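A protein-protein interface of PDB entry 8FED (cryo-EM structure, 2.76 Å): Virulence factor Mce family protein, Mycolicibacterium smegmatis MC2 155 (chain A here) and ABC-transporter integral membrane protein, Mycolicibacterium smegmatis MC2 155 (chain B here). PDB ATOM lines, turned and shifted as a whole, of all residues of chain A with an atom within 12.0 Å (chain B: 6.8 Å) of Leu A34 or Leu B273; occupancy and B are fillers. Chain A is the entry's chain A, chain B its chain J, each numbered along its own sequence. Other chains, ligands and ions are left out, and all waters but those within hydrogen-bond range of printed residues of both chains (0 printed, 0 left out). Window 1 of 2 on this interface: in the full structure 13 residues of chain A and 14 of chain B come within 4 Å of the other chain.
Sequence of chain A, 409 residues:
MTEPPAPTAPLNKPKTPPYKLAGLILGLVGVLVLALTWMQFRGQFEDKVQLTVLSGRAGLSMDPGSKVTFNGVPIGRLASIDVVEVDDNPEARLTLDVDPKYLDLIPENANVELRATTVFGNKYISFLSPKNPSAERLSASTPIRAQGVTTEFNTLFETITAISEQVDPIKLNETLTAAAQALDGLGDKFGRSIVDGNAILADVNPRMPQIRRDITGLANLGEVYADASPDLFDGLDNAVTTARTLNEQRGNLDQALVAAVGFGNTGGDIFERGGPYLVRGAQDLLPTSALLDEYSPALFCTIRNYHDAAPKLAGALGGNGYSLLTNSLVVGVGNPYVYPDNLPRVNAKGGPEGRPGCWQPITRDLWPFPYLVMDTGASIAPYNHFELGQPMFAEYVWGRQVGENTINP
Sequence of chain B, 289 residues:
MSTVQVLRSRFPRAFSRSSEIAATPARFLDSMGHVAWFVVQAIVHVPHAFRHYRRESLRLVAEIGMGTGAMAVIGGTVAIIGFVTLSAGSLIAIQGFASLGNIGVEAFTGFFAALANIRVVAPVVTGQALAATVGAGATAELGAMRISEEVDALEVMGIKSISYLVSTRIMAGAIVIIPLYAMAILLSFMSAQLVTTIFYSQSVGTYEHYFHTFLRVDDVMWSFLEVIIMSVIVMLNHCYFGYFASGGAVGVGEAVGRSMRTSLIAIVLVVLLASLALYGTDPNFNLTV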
ATOM      1  N   ILE A  25      -6.173  11.229  39.610  1.00  0.00           N
ATOM      2  CA  ILE A  25      -5.107  10.271  39.328  1.00  0.00           C
ATOM      3  C   ILE A  25      -5.157   9.823  37.871  1.00  0.00           C
ATOM      4  O   ILE A  25      -4.120   9.718  37.207  1.00  0.00           O
ATOM      5  CB  ILE A  25      -5.190   9.076  40.298  1.00  0.00           C
ATOM      6  CG1 ILE A  25      -4.832   9.519  41.719  1.00  0.00           C
ATOM      7  CG2 ILE A  25      -4.272   7.948  39.854  1.00  0.00           C
ATOM      8  CD1 ILE A  25      -4.936   8.416  42.749  1.00  0.00           C
ATOM      9  N   LEU A  26      -6.360   9.554  37.352  1.00  0.00           N
ATOM     10  CA  LEU A  26      -6.490   9.139  35.956  1.00  0.00           C
ATOM     11  C   LEU A  26      -6.018  10.233  35.006  1.00  0.00           C
ATOM     12  O   LEU A  26      -5.300   9.957  34.034  1.00  0.00           O
ATOM     13  CB  LEU A  26      -7.939   8.759  35.653  1.00  0.00           C
ATOM     14  CG  LEU A  26      -8.246   8.378  34.203  1.00  0.00           C
ATOM     15  CD1 LEU A  26      -7.501   7.113  33.805  1.00  0.00           C
ATOM     16  CD2 LEU A  26      -9.743   8.214  33.986  1.00  0.00           C
ATOM     17  N   GLY A  27      -6.416  11.481  35.266  1.00  0.00           N
ATOM     18  CA  GLY A  27      -5.963  12.581  34.430  1.00  0.00           C
ATOM     19  C   GLY A  27      -4.460  12.776  34.487  1.00  0.00           C
ATOM     20  O   GLY A  27      -3.816  13.019  33.461  1.00  0.00           O
ATOM     21  N   LEU A  28      -3.880  12.668  35.687  1.00  0.00           N
ATOM     22  CA  LEU A  28      -2.434  12.787  35.831  1.00  0.00           C
ATOM     23  C   LEU A  28      -1.714  11.674  35.081  1.00  0.00           C
ATOM     24  O   LEU A  28      -0.687  11.915  34.438  1.00  0.00           O
ATOM     25  CB  LEU A  28      -2.054  12.774  37.311  1.00  0.00           C
ATOM     26  CG  LEU A  28      -0.588  13.046  37.652  1.00  0.00           C
ATOM     27  CD1 LEU A  28      -0.198  14.457  37.243  1.00  0.00           C
ATOM     28  CD2 LEU A  28      -0.330  12.822  39.133  1.00  0.00           C
ATOM     29  N   VAL A  29      -2.242  10.449  35.149  1.00  0.00           N
ATOM     30  CA  VAL A  29      -1.639   9.328  34.434  1.00  0.00           C
ATOM     31  C   VAL A  29      -1.694   9.565  32.931  1.00  0.00           C
ATOM     32  O   VAL A  29      -0.712   9.332  32.217  1.00  0.00           O
ATOM     33  CB  VAL A  29      -2.326   8.007  34.830  1.00  0.00           C
ATOM     34  CG1 VAL A  29      -1.989   6.904  33.839  1.00  0.00           C
ATOM     35  CG2 VAL A  29      -1.903   7.594  36.231  1.00  0.00           C
ATOM     36  N   GLY A  30      -2.838  10.034  32.427  1.00  0.00           N
ATOM     37  CA  GLY A  30      -2.943  10.320  31.003  1.00  0.00           C
ATOM     38  C   GLY A  30      -1.982  11.404  30.548  1.00  0.00           C
ATOM     39  O   GLY A  30      -1.324  11.273  29.510  1.00  0.00           O
ATOM     40  N   VAL A  31      -1.885  12.489  31.322  1.00  0.00           N
ATOM     41  CA  VAL A  31      -0.972  13.576  30.974  1.00  0.00           C
ATOM     42  C   VAL A  31       0.473  13.092  31.004  1.00  0.00           C
ATOM     43  O   VAL A  31       1.276  13.437  30.129  1.00  0.00           O
ATOM     44  CB  VAL A  31      -1.193  14.782  31.907  1.00  0.00           C
ATOM     45  CG1 VAL A  31      -0.115  15.833  31.696  1.00  0.00           C
ATOM     46  CG2 VAL A  31      -2.567  15.388  31.664  1.00  0.00           C
ATOM     47  N   LEU A  32       0.828  12.282  32.007  1.00  0.00           N
ATOM     48  CA  LEU A  32       2.186  11.755  32.089  1.00  0.00           C
ATOM     49  C   LEU A  32       2.495  10.828  30.920  1.00  0.00           C
ATOM     50  O   LEU A  32       3.608  10.847  30.387  1.00  0.00           O
ATOM     51  CB  LEU A  32       2.395  11.033  33.420  1.00  0.00           C
ATOM     52  CG  LEU A  32       3.100  11.825  34.525  1.00  0.00           C
ATOM     53  CD1 LEU A  32       2.346  13.101  34.867  1.00  0.00           C
ATOM     54  CD2 LEU A  32       3.287  10.964  35.767  1.00  0.00           C
ATOM     55  N   VAL A  33       1.526  10.002  30.514  1.00  0.00           N
ATOM     56  CA  VAL A  33       1.733   9.120  29.367  1.00  0.00           C
ATOM     57  C   VAL A  33       1.957   9.936  28.101  1.00  0.00           C
ATOM     58  O   VAL A  33       2.859   9.640  27.304  1.00  0.00           O
ATOM     59  CB  VAL A  33       0.549   8.146  29.217  1.00  0.00           C
ATOM     60  CG1 VAL A  33       0.564   7.486  27.847  1.00  0.00           C
ATOM     61  CG2 VAL A  33       0.596   7.089  30.306  1.00  0.00           C
ATOM     62  N   LEU A  34       1.142  10.976  27.895  1.00  0.00           N
ATOM     63  CA  LEU A  34       1.315  11.823  26.716  1.00  0.00           C
ATOM     64  C   LEU A  34       2.668  12.528  26.735  1.00  0.00           C
ATOM     65  O   LEU A  34       3.352  12.604  25.706  1.00  0.00           O
ATOM     66  CB  LEU A  34       0.176  12.840  26.620  1.00  0.00           C
ATOM     67  CG  LEU A  34      -1.004  12.468  25.716  1.00  0.00           C
ATOM     68  CD1 LEU A  34      -1.743  11.242  26.229  1.00  0.00           C
ATOM     69  CD2 LEU A  34      -1.955  13.645  25.567  1.00  0.00           C
ATOM     70  N   ALA A  35       3.073  13.047  27.896  1.00  0.00           N
ATOM     71  CA  ALA A  35       4.366  13.716  27.994  1.00  0.00           C
ATOM     72  C   ALA A  35       5.511  12.746  27.729  1.00  0.00           C
ATOM     73  O   ALA A  35       6.477  13.091  27.040  1.00  0.00           O
ATOM     74  CB  ALA A  35       4.517  14.367  29.368  1.00  0.00           C
ATOM     75  N   LEU A  36       5.420  11.528  28.270  1.00  0.00           N
ATOM     76  CA  LEU A  36       6.479  10.544  28.070  1.00  0.00           C
ATOM     77  C   LEU A  36       6.586  10.121  26.611  1.00  0.00           C
ATOM     78  O   LEU A  36       7.695   9.996  26.079  1.00  0.00           O
ATOM     79  CB  LEU A  36       6.249   9.329  28.967  1.00  0.00           C
ATOM     80  CG  LEU A  36       7.052   9.276  30.270  1.00  0.00           C
ATOM     81  CD1 LEU A  36       6.810  10.510  31.126  1.00  0.00           C
ATOM     82  CD2 LEU A  36       6.724   8.009  31.045  1.00  0.00           C
ATOM     83  N   THR A  37       5.451   9.890  25.941  1.00  0.00           N
ATOM     84  CA  THR A  37       5.535   9.507  24.535  1.00  0.00           C
ATOM     85  C   THR A  37       6.014  10.667  23.668  1.00  0.00           C
ATOM     86  O   THR A  37       6.737  10.444  22.691  1.00  0.00           O
ATOM     87  CB  THR A  37       4.200   8.943  24.027  1.00  0.00           C
ATOM     88  OG1 THR A  37       4.357   8.498  22.674  1.00  0.00           O
ATOM     89  CG2 THR A  37       3.092   9.970  24.070  1.00  0.00           C
ATOM     90  N   TRP A  38       5.665  11.911  24.021  1.00  0.00           N
ATOM     91  CA  TRP A  38       6.202  13.048  23.279  1.00  0.00           C
ATOM     92  C   TRP A  38       7.709  13.185  23.481  1.00  0.00           C
ATOM     93  O   TRP A  38       8.441  13.483  22.530  1.00  0.00           O
ATOM     94  CB  TRP A  38       5.490  14.336  23.688  1.00  0.00           C
ATOM     95  CG  TRP A  38       6.035  15.548  23.000  1.00  0.00           C
ATOM     96  CD1 TRP A  38       6.740  16.567  23.569  1.00  0.00           C
ATOM     97  CD2 TRP A  38       5.933  15.859  21.606  1.00  0.00           C
ATOM     98  NE1 TRP A  38       7.077  17.498  22.617  1.00  0.00           N
ATOM     99  CE2 TRP A  38       6.593  17.087  21.403  1.00  0.00           C
ATOM    100  CE3 TRP A  38       5.343  15.222  20.510  1.00  0.00           C
ATOM    101  CZ2 TRP A  38       6.680  17.689  20.150  1.00  0.00           C
ATOM    102  CZ3 TRP A  38       5.431  15.820  19.267  1.00  0.00           C
ATOM    103  CH2 TRP A  38       6.094  17.041  19.098  1.00  0.00           C
ATOM    104  N   MET A  39       8.187  12.983  24.712  1.00  0.00           N
ATOM    105  CA  MET A  39       9.624  13.043  24.968  1.00  0.00           C
ATOM    106  C   MET A  39      10.366  11.930  24.239  1.00  0.00           C
ATOM    107  O   MET A  39      11.468  12.144  23.722  1.00  0.00           O
ATOM    108  CB  MET A  39       9.898  12.972  26.471  1.00  0.00           C
ATOM    109  CG  MET A  39       9.502  14.222  27.236  1.00  0.00           C
ATOM    110  SD  MET A  39       9.786  14.063  29.009  1.00  0.00           S
ATOM    111  CE  MET A  39      11.539  13.704  29.040  1.00  0.00           C
ATOM    112  N   GLN A  40       9.783  10.729  24.203  1.00  0.00           N
ATOM    113  CA  GLN A  40      10.375   9.637  23.437  1.00  0.00           C
ATOM    114  C   GLN A  40      10.407   9.961  21.948  1.00  0.00           C
ATOM    115  O   GLN A  40      11.378   9.634  21.255  1.00  0.00           O
ATOM    116  CB  GLN A  40       9.604   8.343  23.698  1.00  0.00           C
ATOM    117  CG  GLN A  40      10.053   7.151  22.866  1.00  0.00           C
ATOM    118  CD  GLN A  40      11.412   6.617  23.273  1.00  0.00           C
ATOM    119  OE1 GLN A  40      11.948   6.973  24.323  1.00  0.00           O
ATOM    120  NE2 GLN A  40      11.978   5.751  22.440  1.00  0.00           N
ATOM    121  N   PHE A  41       9.348  10.597  21.437  1.00  0.00           N
ATOM    122  CA  PHE A  41       9.342  11.030  20.042  1.00  0.00           C
ATOM    123  C   PHE A  41      10.445  12.048  19.776  1.00  0.00           C
ATOM    124  O   PHE A  41      11.130  11.980  18.749  1.00  0.00           O
ATOM    125  CB  PHE A  41       7.972  11.608  19.687  1.00  0.00           C
ATOM    126  CG  PHE A  41       7.916  12.260  18.336  1.00  0.00           C
ATOM    127  CD1 PHE A  41       7.774  11.499  17.191  1.00  0.00           C
ATOM    128  CD2 PHE A  41       7.985  13.638  18.211  1.00  0.00           C
ATOM    129  CE1 PHE A  41       7.718  12.095  15.949  1.00  0.00           C
ATOM    130  CE2 PHE A  41       7.930  14.239  16.971  1.00  0.00           C
ATOM    131  CZ  PHE A  41       7.796  13.466  15.839  1.00  0.00           C
ATOM    132  N   ARG A  42      10.630  12.999  20.690  1.00  0.00           N
ATOM    133  CA  ARG A  42      11.678  14.002  20.564  1.00  0.00           C
ATOM    134  C   ARG A  42      13.063  13.466  20.898  1.00  0.00           C
ATOM    135  O   ARG A  42      14.050  14.177  20.680  1.00  0.00           O
ATOM    136  CB  ARG A  42      11.364  15.203  21.461  1.00  0.00           C
ATOM    137  CG  ARG A  42      10.468  16.246  20.815  1.00  0.00           C
ATOM    138  CD  ARG A  42      11.224  17.028  19.752  1.00  0.00           C
ATOM    139  NE  ARG A  42      10.396  18.048  19.122  1.00  0.00           N
ATOM    140  CZ  ARG A  42       9.813  17.914  17.939  1.00  0.00           C
ATOM    141  NH1 ARG A  42       9.949  16.812  17.222  1.00  0.00           N
ATOM    142  NH2 ARG A  42       9.078  18.914  17.461  1.00  0.00           N
ATOM    143  N   GLY A  43      13.162  12.245  21.412  1.00  0.00           N
ATOM    144  CA  GLY A  43      14.450  11.685  21.791  1.00  0.00           C
ATOM    145  C   GLY A  43      15.114  12.413  22.938  1.00  0.00           C
ATOM    146  O   GLY A  43      16.341  12.571  22.940  1.00  0.00           O
ATOM    147  N   GLN A  44      14.329  12.863  23.919  1.00  0.00           N
ATOM    148  CA  GLN A  44      14.886  13.623  25.034  1.00  0.00           C
ATOM    149  C   GLN A  44      15.673  12.737  25.991  1.00  0.00           C
ATOM    150  O   GLN A  44      16.614  13.212  26.635  1.00  0.00           O
ATOM    151  CB  GLN A  44      13.767  14.346  25.785  1.00  0.00           C
ATOM    152  CG  GLN A  44      12.994  15.351  24.944  1.00  0.00           C
ATOM    153  CD  GLN A  44      13.784  16.616  24.667  1.00  0.00           C
ATOM    154  OE1 GLN A  44      14.780  16.899  25.333  1.00  0.00           O
ATOM    155  NE2 GLN A  44      13.340  17.386  23.680  1.00  0.00           N
ATOM    156  N   PHE A  45      15.300  11.460  26.107  1.00  0.00           N
ATOM    157  CA  PHE A  45      15.930  10.589  27.094  1.00  0.00           C
ATOM    158  C   PHE A  45      17.379  10.292  26.730  1.00  0.00           C
ATOM    159  O   PHE A  45      18.277  10.410  27.571  1.00  0.00           O
ATOM    160  CB  PHE A  45      15.127   9.295  27.237  1.00  0.00           C
ATOM    161  CG  PHE A  45      13.705   9.512  27.665  1.00  0.00           C
ATOM    162  CD1 PHE A  45      13.408   9.863  28.971  1.00  0.00           C
ATOM    163  CD2 PHE A  45      12.666   9.369  26.762  1.00  0.00           C
ATOM    164  CE1 PHE A  45      12.102  10.066  29.369  1.00  0.00           C
ATOM    165  CE2 PHE A  45      11.356   9.570  27.154  1.00  0.00           C
ATOM    166  CZ  PHE A  45      11.075   9.918  28.458  1.00  0.00           C
ATOM    167  N   GLU B 226       0.784  -3.434  20.836  1.00  0.00           N
ATOM    168  CA  GLU B 226      -0.209  -2.380  20.650  1.00  0.00           C
ATOM    169  C   GLU B 226      -1.615  -2.958  20.630  1.00  0.00           C
ATOM    170  O   GLU B 226      -2.529  -2.422  21.264  1.00  0.00           O
ATOM    171  CB  GLU B 226       0.056  -1.614  19.353  1.00  0.00           C
ATOM    172  CG  GLU B 226       1.379  -0.891  19.292  1.00  0.00           C
ATOM    173  CD  GLU B 226       1.655  -0.312  17.918  1.00  0.00           C
ATOM    174  OE1 GLU B 226       0.860  -0.574  16.993  1.00  0.00           O
ATOM    175  OE2 GLU B 226       2.667   0.403  17.762  1.00  0.00           O
ATOM    176  N   VAL B 268      -7.819   4.672  17.726  1.00  0.00           N
ATOM    177  CA  VAL B 268      -6.993   5.498  16.848  1.00  0.00           C
ATOM    178  C   VAL B 268      -5.926   6.233  17.655  1.00  0.00           C
ATOM    179  O   VAL B 268      -4.754   6.288  17.256  1.00  0.00           O
ATOM    180  CB  VAL B 268      -7.869   6.466  16.034  1.00  0.00           C
ATOM    181  CG1 VAL B 268      -7.003   7.312  15.127  1.00  0.00           C
ATOM    182  CG2 VAL B 268      -8.877   5.689  15.209  1.00  0.00           C
ATOM    183  N   LEU B 269      -6.308   6.786  18.812  1.00  0.00           N
ATOM    184  CA  LEU B 269      -5.351   7.524  19.632  1.00  0.00           C
ATOM    185  C   LEU B 269      -4.223   6.625  20.130  1.00  0.00           C
ATOM    186  O   LEU B 269      -3.052   7.026  20.122  1.00  0.00           O
ATOM    187  CB  LEU B 269      -6.075   8.182  20.805  1.00  0.00           C
ATOM    188  CG  LEU B 269      -5.278   9.194  21.626  1.00  0.00           C
ATOM    189  CD1 LEU B 269      -4.786  10.323  20.740  1.00  0.00           C
ATOM    190  CD2 LEU B 269      -6.127   9.733  22.762  1.00  0.00           C
ATOM    191  N   VAL B 270      -4.555   5.408  20.568  1.00  0.00           N
ATOM    192  CA  VAL B 270      -3.544   4.494  21.094  1.00  0.00           C
ATOM    193  C   VAL B 270      -2.560   4.100  20.002  1.00  0.00           C
ATOM    194  O   VAL B 270      -1.340   4.091  20.216  1.00  0.00           O
ATOM    195  CB  VAL B 270      -4.212   3.262  21.732  1.00  0.00           C
ATOM    196  CG1 VAL B 270      -3.213   2.129  21.893  1.00  0.00           C
ATOM    197  CG2 VAL B 270      -4.805   3.629  23.082  1.00  0.00           C
ATOM    198  N   VAL B 271      -3.072   3.765  18.812  1.00  0.00           N
ATOM    199  CA  VAL B 271      -2.178   3.383  17.720  1.00  0.00           C
ATOM    200  C   VAL B 271      -1.273   4.550  17.337  1.00  0.00           C
ATOM    201  O   VAL B 271      -0.068   4.370  17.112  1.00  0.00           O
ATOM    202  CB  VAL B 271      -2.982   2.860  16.516  1.00  0.00           C
ATOM    203  CG1 VAL B 271      -2.052   2.535  15.360  1.00  0.00           C
ATOM    204  CG2 VAL B 271      -3.766   1.623  16.907  1.00  0.00           C
ATOM    205  N   LEU B 272      -1.836   5.764  17.268  1.00  0.00           N
ATOM    206  CA  LEU B 272      -1.029   6.938  16.946  1.00  0.00           C
ATOM    207  C   LEU B 272       0.087   7.142  17.963  1.00  0.00           C
ATOM    208  O   LEU B 272       1.250   7.346  17.593  1.00  0.00           O
ATOM    209  CB  LEU B 272      -1.911   8.184  16.885  1.00  0.00           C
ATOM    210  CG  LEU B 272      -1.131   9.501  16.942  1.00  0.00           C
ATOM    211  CD1 LEU B 272      -0.393   9.745  15.639  1.00  0.00           C
ATOM    212  CD2 LEU B 272      -2.019  10.679  17.292  1.00  0.00           C
ATOM    213  N   LEU B 273      -0.252   7.096  19.256  1.00  0.00           N
ATOM    214  CA  LEU B 273       0.749   7.335  20.293  1.00  0.00           C
ATOM    215  C   LEU B 273       1.839   6.272  20.267  1.00  0.00           C
ATOM    216  O   LEU B 273       3.028   6.588  20.397  1.00  0.00           O
ATOM    217  CB  LEU B 273       0.086   7.388  21.667  1.00  0.00           C
ATOM    218  CG  LEU B 273      -0.803   8.600  21.951  1.00  0.00           C
ATOM    219  CD1 LEU B 273      -1.309   8.567  23.382  1.00  0.00           C
ATOM    220  CD2 LEU B 273      -0.056   9.895  21.675  1.00  0.00           C
ATOM    221  N   ALA B 274       1.453   5.005  20.097  1.00  0.00           N
ATOM    222  CA  ALA B 274       2.440   3.931  20.075  1.00  0.00           C
ATOM    223  C   ALA B 274       3.380   4.057  18.883  1.00  0.00           C
ATOM    224  O   ALA B 274       4.599   3.897  19.027  1.00  0.00           O
ATOM    225  CB  ALA B 274       1.734   2.578  20.065  1.00  0.00           C
ATOM    226  N   SER B 275       2.837   4.346  17.696  1.00  0.00           N
ATOM    227  CA  SER B 275       3.687   4.500  16.518  1.00  0.00           C
ATOM    228  C   SER B 275       4.597   5.717  16.637  1.00  0.00           C
ATOM    229  O   SER B 275       5.745   5.683  16.181  1.00  0.00           O
ATOM    230  CB  SER B 275       2.833   4.590  15.258  1.00  0.00           C
ATOM    231  OG  SER B 275       2.175   3.363  15.001  1.00  0.00           O
ATOM    232  N   LEU B 276       4.100   6.806  17.229  1.00  0.00           N
ATOM    233  CA  LEU B 276       4.947   7.975  17.445  1.00  0.00           C
ATOM    234  C   LEU B 276       6.070   7.675  18.430  1.00  0.00           C
ATOM    235  O   LEU B 276       7.192   8.164  18.267  1.00  0.00           O
ATOM    236  CB  LEU B 276       4.107   9.153  17.934  1.00  0.00           C
ATOM    237  CG  LEU B 276       3.928  10.300  16.940  1.00  0.00           C
ATOM    238  CD1 LEU B 276       3.291   9.798  15.658  1.00  0.00           C
ATOM    239  CD2 LEU B 276       3.097  11.410  17.554  1.00  0.00           C
ATOM    240  N   ALA B 277       5.783   6.887  19.469  1.00  0.00           N
ATOM    241  CA  ALA B 277       6.806   6.580  20.461  1.00  0.00           C
ATOM    242  C   ALA B 277       7.867   5.643  19.895  1.00  0.00           C
ATOM    243  O   ALA B 277       9.068   5.864  20.087  1.00  0.00           O
ATOM    244  CB  ALA B 277       6.164   5.969  21.705  1.00  0.00           C
ATOM    245  N   LEU B 278       7.444   4.591  19.193  1.00  0.00           N
ATOM    246  CA  LEU B 278       8.389   3.566  18.760  1.00  0.00           C
ATOM    247  C   LEU B 278       9.318   4.078  17.665  1.00  0.00           C
ATOM    248  O   LEU B 278      10.537   3.890  17.736  1.00  0.00           O
ATOM    249  CB  LEU B 278       7.631   2.329  18.285  1.00  0.00           C
ATOM    250  CG  LEU B 278       6.887   1.565  19.379  1.00  0.00           C
ATOM    251  CD1 LEU B 278       5.946   0.554  18.761  1.00  0.00           C
ATOM    252  CD2 LEU B 278       7.870   0.886  20.316  1.00  0.00           C
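OG1 of Thr A37 sits at hydrogen-bond distance from O of Leu B273.
Leu A34 touches just one residue of chain B: Leu B273. Of chain A, only Leu A34 and Thr A37 come within 4 Å of Leu B273. No residue of chain A comes within 4 Å of Leu B272. No residue of chain A comes within 4 Å of Ala B274. No residue of chain A comes within 4 Å of Ser B275. Leu B276 touches just one residue of chain A: Phe A41. Of the printed residues of chain B, Gln A40 touches Ala B277 (3.2 Å). Printed residues of chain B within 4 Å of Phe A41: Leu B276. Of the printed residues of chain B, Thr A37 touches Leu B273 (3.3 Å) and Ala B277 (3.3 Å). The nearest residue of chain A that does not touch Leu B273 is Val A33 (5.0 Å).
Leu B273 touches Leu A34. Thr A37 touches Ala B277. CG of Gln A40 touches O of Ala B277 (3.2 Å). CD1 of Phe A41 touches O of Leu B276 (3.6 Å).
Of the 21 printed residues of chain A, 4 touch a printed residue of chain B. Printed residues of chain A that touch a printed residue of chain B: Leu A34, Thr A37, Gln A40 and Phe A41. Hydrophobic or aromatic side chains of chain B that line the printed part of chain A: Leu B273 and Ala B277. Among the printed residues, 5 pairs touch across the chains. Among the printed residues, no Asp or Glu carboxylate lies within 4 Å of a Lys or Arg side-chain nitrogen of the other chain.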
